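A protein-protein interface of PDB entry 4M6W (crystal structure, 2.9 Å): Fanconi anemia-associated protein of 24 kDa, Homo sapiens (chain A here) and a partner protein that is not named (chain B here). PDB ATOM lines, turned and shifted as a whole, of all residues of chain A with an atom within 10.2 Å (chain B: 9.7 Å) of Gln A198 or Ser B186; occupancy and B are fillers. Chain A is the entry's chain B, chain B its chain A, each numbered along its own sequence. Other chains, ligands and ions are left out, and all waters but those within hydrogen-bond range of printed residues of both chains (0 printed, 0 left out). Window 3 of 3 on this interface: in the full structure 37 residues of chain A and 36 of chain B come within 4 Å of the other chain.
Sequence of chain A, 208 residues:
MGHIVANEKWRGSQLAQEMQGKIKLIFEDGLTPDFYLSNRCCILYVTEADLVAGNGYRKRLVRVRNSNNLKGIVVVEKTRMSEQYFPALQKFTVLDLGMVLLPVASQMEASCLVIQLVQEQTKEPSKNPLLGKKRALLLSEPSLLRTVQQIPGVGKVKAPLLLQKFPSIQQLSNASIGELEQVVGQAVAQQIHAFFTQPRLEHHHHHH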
ATOM      1  N   ILE A 169      32.979  -9.812 -26.094  1.00  0.00           N
ATOM      2  CA  ILE A 169      32.358  -8.480 -26.189  1.00  0.00           C
ATOM      3  C   ILE A 169      33.377  -7.416 -25.754  1.00  0.00           C
ATOM      4  O   ILE A 169      33.386  -6.299 -26.279  1.00  0.00           O
ATOM      5  CB  ILE A 169      31.049  -8.375 -25.348  1.00  0.00           C
ATOM      6  CG1 ILE A 169      29.989  -9.361 -25.867  1.00  0.00           C
ATOM      7  CG2 ILE A 169      30.476  -6.958 -25.388  1.00  0.00           C
ATOM      8  CD1 ILE A 169      28.794  -9.543 -24.951  1.00  0.00           C
ATOM      9  N   SER A 173      34.655  -4.466 -28.084  1.00  0.00           N
ATOM     10  CA  SER A 173      34.485  -3.079 -27.641  1.00  0.00           C
ATOM     11  C   SER A 173      35.703  -2.212 -27.957  1.00  0.00           C
ATOM     12  O   SER A 173      35.564  -1.116 -28.510  1.00  0.00           O
ATOM     13  CB  SER A 173      34.180  -3.022 -26.143  1.00  0.00           C
ATOM     14  OG  SER A 173      35.295  -3.423 -25.370  1.00  0.00           O
ATOM     15  N   ASN A 174      36.891  -2.703 -27.609  1.00  0.00           N
ATOM     16  CA  ASN A 174      38.141  -2.006 -27.940  1.00  0.00           C
ATOM     17  C   ASN A 174      38.771  -2.549 -29.232  1.00  0.00           C
ATOM     18  O   ASN A 174      39.937  -2.947 -29.252  1.00  0.00           O
ATOM     19  CB  ASN A 174      39.139  -1.999 -26.756  1.00  0.00           C
ATOM     20  CG  ASN A 174      39.152  -3.299 -25.966  1.00  0.00           C
ATOM     21  OD1 ASN A 174      39.142  -4.388 -26.536  1.00  0.00           O
ATOM     22  ND2 ASN A 174      39.183  -3.187 -24.642  1.00  0.00           N
ATOM     23  N   GLN A 191      30.008   1.764 -37.977  1.00  0.00           N
ATOM     24  CA  GLN A 191      28.738   1.709 -37.233  1.00  0.00           C
ATOM     25  C   GLN A 191      28.884   0.956 -35.898  1.00  0.00           C
ATOM     26  O   GLN A 191      28.171   1.240 -34.931  1.00  0.00           O
ATOM     27  CB  GLN A 191      27.657   1.042 -38.100  1.00  0.00           C
ATOM     28  CG  GLN A 191      26.229   1.493 -37.828  1.00  0.00           C
ATOM     29  CD  GLN A 191      25.242   1.015 -38.888  1.00  0.00           C
ATOM     30  OE1 GLN A 191      25.627   0.417 -39.895  1.00  0.00           O
ATOM     31  NE2 GLN A 191      23.959   1.280 -38.661  1.00  0.00           N
ATOM     32  N   ILE A 192      29.802  -0.009 -35.861  1.00  0.00           N
ATOM     33  CA  ILE A 192      30.103  -0.764 -34.645  1.00  0.00           C
ATOM     34  C   ILE A 192      31.001   0.049 -33.703  1.00  0.00           C
ATOM     35  O   ILE A 192      30.792   0.044 -32.492  1.00  0.00           O
ATOM     36  CB  ILE A 192      30.762  -2.124 -34.982  1.00  0.00           C
ATOM     37  CG1 ILE A 192      29.791  -2.998 -35.785  1.00  0.00           C
ATOM     38  CG2 ILE A 192      31.169  -2.872 -33.717  1.00  0.00           C
ATOM     39  CD1 ILE A 192      30.460  -4.103 -36.576  1.00  0.00           C
ATOM     40  N   HIS A 193      31.995   0.743 -34.258  1.00  0.00           N
ATOM     41  CA  HIS A 193      32.897   1.594 -33.459  1.00  0.00           C
ATOM     42  C   HIS A 193      32.167   2.825 -32.905  1.00  0.00           C
ATOM     43  O   HIS A 193      32.453   3.265 -31.791  1.00  0.00           O
ATOM     44  CB  HIS A 193      34.127   2.026 -34.283  1.00  0.00           C
ATOM     45  CG  HIS A 193      35.247   2.601 -33.464  1.00  0.00           C
ATOM     46  ND1 HIS A 193      35.369   3.950 -33.206  1.00  0.00           N
ATOM     47  CD2 HIS A 193      36.306   2.009 -32.862  1.00  0.00           C
ATOM     48  CE1 HIS A 193      36.448   4.162 -32.473  1.00  0.00           C
ATOM     49  NE2 HIS A 193      37.036   3.002 -32.251  1.00  0.00           N
ATOM     50  N   ALA A 194      31.232   3.374 -33.681  1.00  0.00           N
ATOM     51  CA  ALA A 194      30.427   4.514 -33.229  1.00  0.00           C
ATOM     52  C   ALA A 194      29.499   4.124 -32.073  1.00  0.00           C
ATOM     53  O   ALA A 194      29.269   4.921 -31.165  1.00  0.00           O
ATOM     54  CB  ALA A 194      29.622   5.094 -34.385  1.00  0.00           C
ATOM     55  N   PHE A 195      28.981   2.897 -32.113  1.00  0.00           N
ATOM     56  CA  PHE A 195      28.139   2.360 -31.035  1.00  0.00           C
ATOM     57  C   PHE A 195      28.891   2.333 -29.698  1.00  0.00           C
ATOM     58  O   PHE A 195      28.377   2.806 -28.687  1.00  0.00           O
ATOM     59  CB  PHE A 195      27.631   0.956 -31.416  1.00  0.00           C
ATOM     60  CG  PHE A 195      26.899   0.236 -30.311  1.00  0.00           C
ATOM     61  CD1 PHE A 195      25.589   0.564 -29.994  1.00  0.00           C
ATOM     62  CD2 PHE A 195      27.516  -0.791 -29.606  1.00  0.00           C
ATOM     63  CE1 PHE A 195      24.914  -0.103 -28.986  1.00  0.00           C
ATOM     64  CE2 PHE A 195      26.847  -1.460 -28.596  1.00  0.00           C
ATOM     65  CZ  PHE A 195      25.543  -1.116 -28.286  1.00  0.00           C
ATOM     66  N   PHE A 196      30.110   1.801 -29.708  1.00  0.00           N
ATOM     67  CA  PHE A 196      30.917   1.673 -28.488  1.00  0.00           C
ATOM     68  C   PHE A 196      31.481   3.009 -27.977  1.00  0.00           C
ATOM     69  O   PHE A 196      31.482   3.255 -26.772  1.00  0.00           O
ATOM     70  CB  PHE A 196      32.051   0.652 -28.689  1.00  0.00           C
ATOM     71  CG  PHE A 196      31.598  -0.789 -28.642  1.00  0.00           C
ATOM     72  CD1 PHE A 196      31.095  -1.339 -27.467  1.00  0.00           C
ATOM     73  CD2 PHE A 196      31.699  -1.601 -29.761  1.00  0.00           C
ATOM     74  CE1 PHE A 196      30.686  -2.662 -27.417  1.00  0.00           C
ATOM     75  CE2 PHE A 196      31.294  -2.924 -29.716  1.00  0.00           C
ATOM     76  CZ  PHE A 196      30.789  -3.456 -28.543  1.00  0.00           C
ATOM     77  N   THR A 197      31.954   3.863 -28.884  1.00  0.00           N
ATOM     78  CA  THR A 197      32.517   5.172 -28.513  1.00  0.00           C
ATOM     79  C   THR A 197      31.406   6.176 -28.160  1.00  0.00           C
ATOM     80  O   THR A 197      30.463   6.374 -28.931  1.00  0.00           O
ATOM     81  CB  THR A 197      33.412   5.738 -29.643  1.00  0.00           C
ATOM     82  OG1 THR A 197      34.466   4.808 -29.931  1.00  0.00           O
ATOM     83  CG2 THR A 197      34.029   7.092 -29.260  1.00  0.00           C
ATOM     84  N   GLN A 198      31.539   6.803 -26.989  1.00  0.00           N
ATOM     85  CA  GLN A 198      30.518   7.700 -26.426  1.00  0.00           C
ATOM     86  C   GLN A 198      29.143   7.026 -26.411  1.00  0.00           C
ATOM     87  O   GLN A 198      29.028   5.833 -26.119  1.00  0.00           O
ATOM     88  CB  GLN A 198      30.464   9.036 -27.185  1.00  0.00           C
ATOM     89  CG  GLN A 198      30.098  10.239 -26.316  1.00  0.00           C
ATOM     90  CD  GLN A 198      28.685  10.171 -25.752  1.00  0.00           C
ATOM     91  OE1 GLN A 198      27.732   9.867 -26.474  1.00  0.00           O
ATOM     92  NE2 GLN A 198      28.540  10.460 -24.456  1.00  0.00           N
ATOM     93  N   SER B 160      18.117   7.857 -26.041  1.00  0.00           N
ATOM     94  CA  SER B 160      19.138   6.825 -25.858  1.00  0.00           C
ATOM     95  C   SER B 160      18.571   5.428 -26.161  1.00  0.00           C
ATOM     96  O   SER B 160      17.550   5.035 -25.595  1.00  0.00           O
ATOM     97  CB  SER B 160      19.693   6.885 -24.429  1.00  0.00           C
ATOM     98  OG  SER B 160      20.818   6.039 -24.266  1.00  0.00           O
ATOM     99  N   ALA B 162      20.792   2.409 -26.556  1.00  0.00           N
ATOM    100  CA  ALA B 162      21.716   1.318 -26.210  1.00  0.00           C
ATOM    101  C   ALA B 162      21.066   0.410 -25.161  1.00  0.00           C
ATOM    102  O   ALA B 162      21.680  -0.547 -24.682  1.00  0.00           O
ATOM    103  CB  ALA B 162      23.027   1.879 -25.680  1.00  0.00           C
ATOM    104  N   PHE B 165      20.628  -3.428 -26.210  1.00  0.00           N
ATOM    105  CA  PHE B 165      21.872  -4.185 -26.024  1.00  0.00           C
ATOM    106  C   PHE B 165      22.020  -4.700 -24.586  1.00  0.00           C
ATOM    107  O   PHE B 165      22.406  -5.849 -24.379  1.00  0.00           O
ATOM    108  CB  PHE B 165      23.093  -3.333 -26.415  1.00  0.00           C
ATOM    109  CG  PHE B 165      24.424  -3.987 -26.127  1.00  0.00           C
ATOM    110  CD1 PHE B 165      25.052  -3.810 -24.898  1.00  0.00           C
ATOM    111  CD2 PHE B 165      25.055  -4.763 -27.085  1.00  0.00           C
ATOM    112  CE1 PHE B 165      26.277  -4.405 -24.628  1.00  0.00           C
ATOM    113  CE2 PHE B 165      26.282  -5.358 -26.822  1.00  0.00           C
ATOM    114  CZ  PHE B 165      26.893  -5.179 -25.591  1.00  0.00           C
ATOM    115  N   TYR B 166      21.731  -3.850 -23.601  1.00  0.00           N
ATOM    116  CA  TYR B 166      21.794  -4.263 -22.191  1.00  0.00           C
ATOM    117  C   TYR B 166      20.651  -5.216 -21.837  1.00  0.00           C
ATOM    118  O   TYR B 166      20.815  -6.092 -20.988  1.00  0.00           O
ATOM    119  CB  TYR B 166      21.772  -3.051 -21.249  1.00  0.00           C
ATOM    120  CG  TYR B 166      22.994  -2.159 -21.332  1.00  0.00           C
ATOM    121  CD1 TYR B 166      24.269  -2.662 -21.076  1.00  0.00           C
ATOM    122  CD2 TYR B 166      22.875  -0.808 -21.649  1.00  0.00           C
ATOM    123  CE1 TYR B 166      25.391  -1.846 -21.149  1.00  0.00           C
ATOM    124  CE2 TYR B 166      23.990   0.017 -21.721  1.00  0.00           C
ATOM    125  CZ  TYR B 166      25.246  -0.506 -21.469  1.00  0.00           C
ATOM    126  OH  TYR B 166      26.356   0.308 -21.537  1.00  0.00           O
ATOM    127  N   MET B 180      22.230   1.135 -16.390  1.00  0.00           N
ATOM    128  CA  MET B 180      23.473   0.778 -17.079  1.00  0.00           C
ATOM    129  C   MET B 180      23.700   1.770 -18.225  1.00  0.00           C
ATOM    130  O   MET B 180      24.836   2.146 -18.505  1.00  0.00           O
ATOM    131  CB  MET B 180      23.440  -0.667 -17.615  1.00  0.00           C
ATOM    132  CG  MET B 180      23.702  -1.742 -16.566  1.00  0.00           C
ATOM    133  SD  MET B 180      23.654  -3.430 -17.208  1.00  0.00           S
ATOM    134  CE  MET B 180      25.356  -3.677 -17.681  1.00  0.00           C
ATOM    135  N   CYS B 181      22.620   2.191 -18.886  1.00  0.00           N
ATOM    136  CA  CYS B 181      22.704   3.225 -19.922  1.00  0.00           C
ATOM    137  C   CYS B 181      23.173   4.535 -19.302  1.00  0.00           C
ATOM    138  O   CYS B 181      24.131   5.147 -19.777  1.00  0.00           O
ATOM    139  CB  CYS B 181      21.352   3.422 -20.612  1.00  0.00           C
ATOM    140  SG  CYS B 181      20.759   1.964 -21.497  1.00  0.00           S
ATOM    141  N   HIS B 182      22.493   4.951 -18.233  1.00  0.00           N
ATOM    142  CA  HIS B 182      22.954   6.052 -17.382  1.00  0.00           C
ATOM    143  C   HIS B 182      24.068   5.476 -16.499  1.00  0.00           C
ATOM    144  O   HIS B 182      24.240   4.258 -16.437  1.00  0.00           O
ATOM    145  CB  HIS B 182      21.793   6.601 -16.528  1.00  0.00           C
ATOM    146  CG  HIS B 182      21.822   8.090 -16.320  1.00  0.00           C
ATOM    147  ND1 HIS B 182      21.640   8.993 -17.348  1.00  0.00           N
ATOM    148  CD2 HIS B 182      21.969   8.832 -15.194  1.00  0.00           C
ATOM    149  CE1 HIS B 182      21.697  10.225 -16.868  1.00  0.00           C
ATOM    150  NE2 HIS B 182      21.893  10.154 -15.564  1.00  0.00           N
ATOM    151  N   GLN B 183      24.839   6.345 -15.850  1.00  0.00           N
ATOM    152  CA  GLN B 183      25.939   5.935 -14.952  1.00  0.00           C
ATOM    153  C   GLN B 183      27.156   5.283 -15.651  1.00  0.00           C
ATOM    154  O   GLN B 183      28.222   5.176 -15.050  1.00  0.00           O
ATOM    155  CB  GLN B 183      25.420   5.049 -13.801  1.00  0.00           C
ATOM    156  CG  GLN B 183      24.316   5.704 -12.974  1.00  0.00           C
ATOM    157  CD  GLN B 183      24.056   5.001 -11.648  1.00  0.00           C
ATOM    158  OE1 GLN B 183      24.991   4.698 -10.899  1.00  0.00           O
ATOM    159  NE2 GLN B 183      22.781   4.753 -11.342  1.00  0.00           N
ATOM    160  N   PHE B 184      27.001   4.847 -16.901  1.00  0.00           N
ATOM    161  CA  PHE B 184      28.134   4.416 -17.725  1.00  0.00           C
ATOM    162  C   PHE B 184      28.278   5.364 -18.914  1.00  0.00           C
ATOM    163  O   PHE B 184      27.337   5.538 -19.692  1.00  0.00           O
ATOM    164  CB  PHE B 184      27.946   2.982 -18.230  1.00  0.00           C
ATOM    165  CG  PHE B 184      28.277   1.923 -17.213  1.00  0.00           C
ATOM    166  CD1 PHE B 184      29.594   1.697 -16.834  1.00  0.00           C
ATOM    167  CD2 PHE B 184      27.279   1.137 -16.649  1.00  0.00           C
ATOM    168  CE1 PHE B 184      29.908   0.719 -15.903  1.00  0.00           C
ATOM    169  CE2 PHE B 184      27.587   0.157 -15.719  1.00  0.00           C
ATOM    170  CZ  PHE B 184      28.903  -0.052 -15.346  1.00  0.00           C
ATOM    171  N   SER B 185      29.459   5.971 -19.040  1.00  0.00           N
ATOM    172  CA  SER B 185      29.747   6.938 -20.106  1.00  0.00           C
ATOM    173  C   SER B 185      29.718   6.294 -21.497  1.00  0.00           C
ATOM    174  O   SER B 185      29.191   6.873 -22.448  1.00  0.00           O
ATOM    175  CB  SER B 185      31.109   7.594 -19.858  1.00  0.00           C
ATOM    176  OG  SER B 185      32.098   6.613 -19.587  1.00  0.00           O
ATOM    177  N   SER B 186      30.289   5.097 -21.598  1.00  0.00           N
ATOM    178  CA  SER B 186      30.294   4.324 -22.837  1.00  0.00           C
ATOM    179  C   SER B 186      29.978   2.857 -22.560  1.00  0.00           C
ATOM    180  O   SER B 186      30.325   2.324 -21.500  1.00  0.00           O
ATOM    181  CB  SER B 186      31.665   4.420 -23.510  1.00  0.00           C
ATOM    182  OG  SER B 186      31.923   5.738 -23.962  1.00  0.00           O
ATOM    183  N   VAL B 187      29.315   2.211 -23.517  1.00  0.00           N
ATOM    184  CA  VAL B 187      29.155   0.751 -23.495  1.00  0.00           C
ATOM    185  C   VAL B 187      30.538   0.107 -23.667  1.00  0.00           C
ATOM    186  O   VAL B 187      30.777  -1.007 -23.191  1.00  0.00           O
ATOM    187  CB  VAL B 187      28.107   0.243 -24.534  1.00  0.00           C
ATOM    188  CG1 VAL B 187      28.365   0.801 -25.925  1.00  0.00           C
ATOM    189  CG2 VAL B 187      28.050  -1.283 -24.584  1.00  0.00           C
ATOM    190  N   LYS B 188      31.445   0.834 -24.324  1.00  0.00           N
ATOM    191  CA  LYS B 188      32.868   0.471 -24.391  1.00  0.00           C
ATOM    192  C   LYS B 188      33.501   0.402 -22.997  1.00  0.00           C
ATOM    193  O   LYS B 188      34.177  -0.576 -22.670  1.00  0.00           O
ATOM    194  CB  LYS B 188      33.635   1.477 -25.268  1.00  0.00           C
ATOM    195  CG  LYS B 188      35.154   1.293 -25.326  1.00  0.00           C
ATOM    196  CD  LYS B 188      35.841   2.493 -25.974  1.00  0.00           C
ATOM    197  CE  LYS B 188      37.354   2.463 -25.791  1.00  0.00           C
ATOM    198  NZ  LYS B 188      38.012   1.386 -26.587  1.00  0.00           N
ATOM    199  N   ARG B 189      33.287   1.443 -22.188  1.00  0.00           N
ATOM    200  CA  ARG B 189      33.871   1.513 -20.842  1.00  0.00           C
ATOM    201  C   ARG B 189      33.153   0.563 -19.885  1.00  0.00           C
ATOM    202  O   ARG B 189      33.760   0.049 -18.945  1.00  0.00           O
ATOM    203  CB  ARG B 189      33.852   2.946 -20.288  1.00  0.00           C
ATOM    204  CG  ARG B 189      34.971   3.221 -19.287  1.00  0.00           C
ATOM    205  CD  ARG B 189      34.650   4.378 -18.344  1.00  0.00           C
ATOM    206  NE  ARG B 189      35.711   4.606 -17.349  1.00  0.00           N
ATOM    207  CZ  ARG B 189      36.638   5.567 -17.402  1.00  0.00           C
ATOM    208  NH1 ARG B 189      36.679   6.441 -18.409  1.00  0.00           N
ATOM    209  NH2 ARG B 189      37.542   5.661 -16.428  1.00  0.00           N
ATOM    210  N   MET B 190      31.862   0.339 -20.131  1.00  0.00           N
ATOM    211  CA  MET B 190      31.082  -0.689 -19.424  1.00  0.00           C
ATOM    212  C   MET B 190      31.709  -2.069 -19.616  1.00  0.00           C
ATOM    213  O   MET B 190      31.796  -2.857 -18.672  1.00  0.00           O
ATOM    214  CB  MET B 190      29.634  -0.697 -19.939  1.00  0.00           C
ATOM    215  CG  MET B 190      28.644  -1.566 -19.162  1.00  0.00           C
ATOM    216  SD  MET B 190      28.738  -3.361 -19.395  1.00  0.00           S
ATOM    217  CE  MET B 190      28.789  -3.537 -21.177  1.00  0.00           C
ATOM    218  N   ALA B 191      32.148  -2.348 -20.842  1.00  0.00           N
ATOM    219  CA  ALA B 191      32.764  -3.631 -21.184  1.00  0.00           C
ATOM    220  C   ALA B 191      34.150  -3.836 -20.563  1.00  0.00           C
ATOM    221  O   ALA B 191      34.606  -4.973 -20.439  1.00  0.00           O
ATOM    222  CB  ALA B 191      32.846  -3.783 -22.697  1.00  0.00           C
ATOM    223  N   ASN B 192      34.815  -2.741 -20.191  1.00  0.00           N
ATOM    224  CA  ASN B 192      36.155  -2.794 -19.600  1.00  0.00           C
ATOM    225  C   ASN B 192      36.193  -2.376 -18.124  1.00  0.00           C
ATOM    226  O   ASN B 192      37.265  -2.122 -17.578  1.00  0.00           O
ATOM    227  CB  ASN B 192      37.116  -1.932 -20.425  1.00  0.00           C
ATOM    228  CG  ASN B 192      37.367  -2.507 -21.811  1.00  0.00           C
ATOM    229  OD1 ASN B 192      38.028  -3.537 -21.951  1.00  0.00           O
ATOM    230  ND2 ASN B 192      36.843  -1.844 -22.841  1.00  0.00           N
ATOM    231  N   SER B 193      35.026  -2.332 -17.485  1.00  0.00           N
ATOM    232  CA  SER B 193      34.911  -1.956 -16.072  1.00  0.00           C
ATOM    233  C   SER B 193      35.170  -3.138 -15.127  1.00  0.00           C
ATOM    234  O   SER B 193      34.733  -4.257 -15.397  1.00  0.00           O
ATOM    235  CB  SER B 193      33.520  -1.376 -15.809  1.00  0.00           C
ATOM    236  OG  SER B 193      33.352  -0.138 -16.478  1.00  0.00           O
ATOM    237  N   GLU B 197      33.144  -1.637  -9.877  1.00  0.00           N
ATOM    238  CA  GLU B 197      32.415  -0.475 -10.398  1.00  0.00           C
ATOM    239  C   GLU B 197      31.180  -0.831 -11.233  1.00  0.00           C
ATOM    240  O   GLU B 197      30.281  -0.004 -11.360  1.00  0.00           O
ATOM    241  CB  GLU B 197      33.346   0.488 -11.158  1.00  0.00           C
ATOM    242  CG  GLU B 197      34.014  -0.062 -12.409  1.00  0.00           C
ATOM    243  CD  GLU B 197      35.062   0.883 -12.982  1.00  0.00           C
ATOM    244  OE1 GLU B 197      35.014   1.165 -14.200  1.00  0.00           O
ATOM    245  OE2 GLU B 197      35.933   1.347 -12.215  1.00  0.00           O
ATOM    246  N   TYR B 201      27.799   0.968 -10.263  1.00  0.00           N
ATOM    247  CA  TYR B 201      27.187   1.779 -11.323  1.00  0.00           C
ATOM    248  C   TYR B 201      25.938   1.128 -11.928  1.00  0.00           C
ATOM    249  O   TYR B 201      24.976   1.826 -12.240  1.00  0.00           O
ATOM    250  CB  TYR B 201      28.199   2.119 -12.432  1.00  0.00           C
ATOM    251  CG  TYR B 201      29.303   3.085 -12.026  1.00  0.00           C
ATOM    252  CD1 TYR B 201      29.014   4.270 -11.347  1.00  0.00           C
ATOM    253  CD2 TYR B 201      30.632   2.832 -12.355  1.00  0.00           C
ATOM    254  CE1 TYR B 201      30.019   5.153 -10.985  1.00  0.00           C
ATOM    255  CE2 TYR B 201      31.643   3.715 -11.997  1.00  0.00           C
ATOM    256  CZ  TYR B 201      31.331   4.872 -11.314  1.00  0.00           C
ATOM    257  OH  TYR B 201      32.330   5.749 -10.959  1.00  0.00           O
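The side-chain hydroxyl of Ser B186 is in hydrogen-bond range of the backbone NH of Gln A198, at 3.2 Å. The backbone NH (N) of Lys B188 sits close to the backbone carbonyl oxygen (O) of Phe A196, at 3.4 Å. The side-chain hydroxyl (OG) of Ser A173 sits at hydrogen-bond distance from the side-chain amide nitrogen (ND2) of Asn B192. The side-chain amide nitrogen (ND2) of Asn A174 sits at hydrogen-bond distance from the side-chain amide oxygen (OD1) of Asn B192.
Ser A173 touches Lys B188 (O to NZ, 3.99 Å). OG of Ser A173 touches CB of Ala B191 (3.6 Å). CB of Asn A174 touches NZ of Lys B188, at 3.6 Å. Phe A195 touches Phe B165. Phe A195 touches Val B187 (O to CG1, 3.4 Å). Ser B186 touches Phe A196. CA of Phe A196 touches CG1 of Val B187, at 3.7 Å. O of Gln A198 touches O of Ser B185 (3.8 Å).
ND2 of Asn B192 sits at hydrogen-bond distance from O of Lys B188.
Of the 11 printed residues of chain A, 5 touch a printed residue of chain B. Among the printed residues, 12 pairs touch across the chains.
Printed residues of chain B within 4 Å of Asn A174: Lys B188 (3.6 Å) and Asn B192 (2.9 Å). Of the printed residues of chain B, Phe A196 touches Ser B186 (3.5 Å), Val B187 (3.7 Å) and Lys B188 (3.2 Å). No residue of chain B comes within 4 Å of Thr A197. Printed residues of chain B within 4 Å of Gln A198: Ser B185 and Ser B186. Of chain A, only Phe A196 and Gln A198 come within 4 Å of Ser B186. Of chain A, only Phe A195 (3.4 Å) and Phe A196 (3.7 Å) come within 4 Å of Val B187. Of the printed residues of chain A, Ala B191 touches Ser A173 (3.6 Å). The nearest residue of chain B that does not touch Gln A198 is Val B187 (4.5 Å). The nearest residue of chain A that does not touch Ser B186 is Thr A197 (4.3 Å). The nearest printed residue of chain B that does not touch Phe A195 is Ala B162 (4.3 Å).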
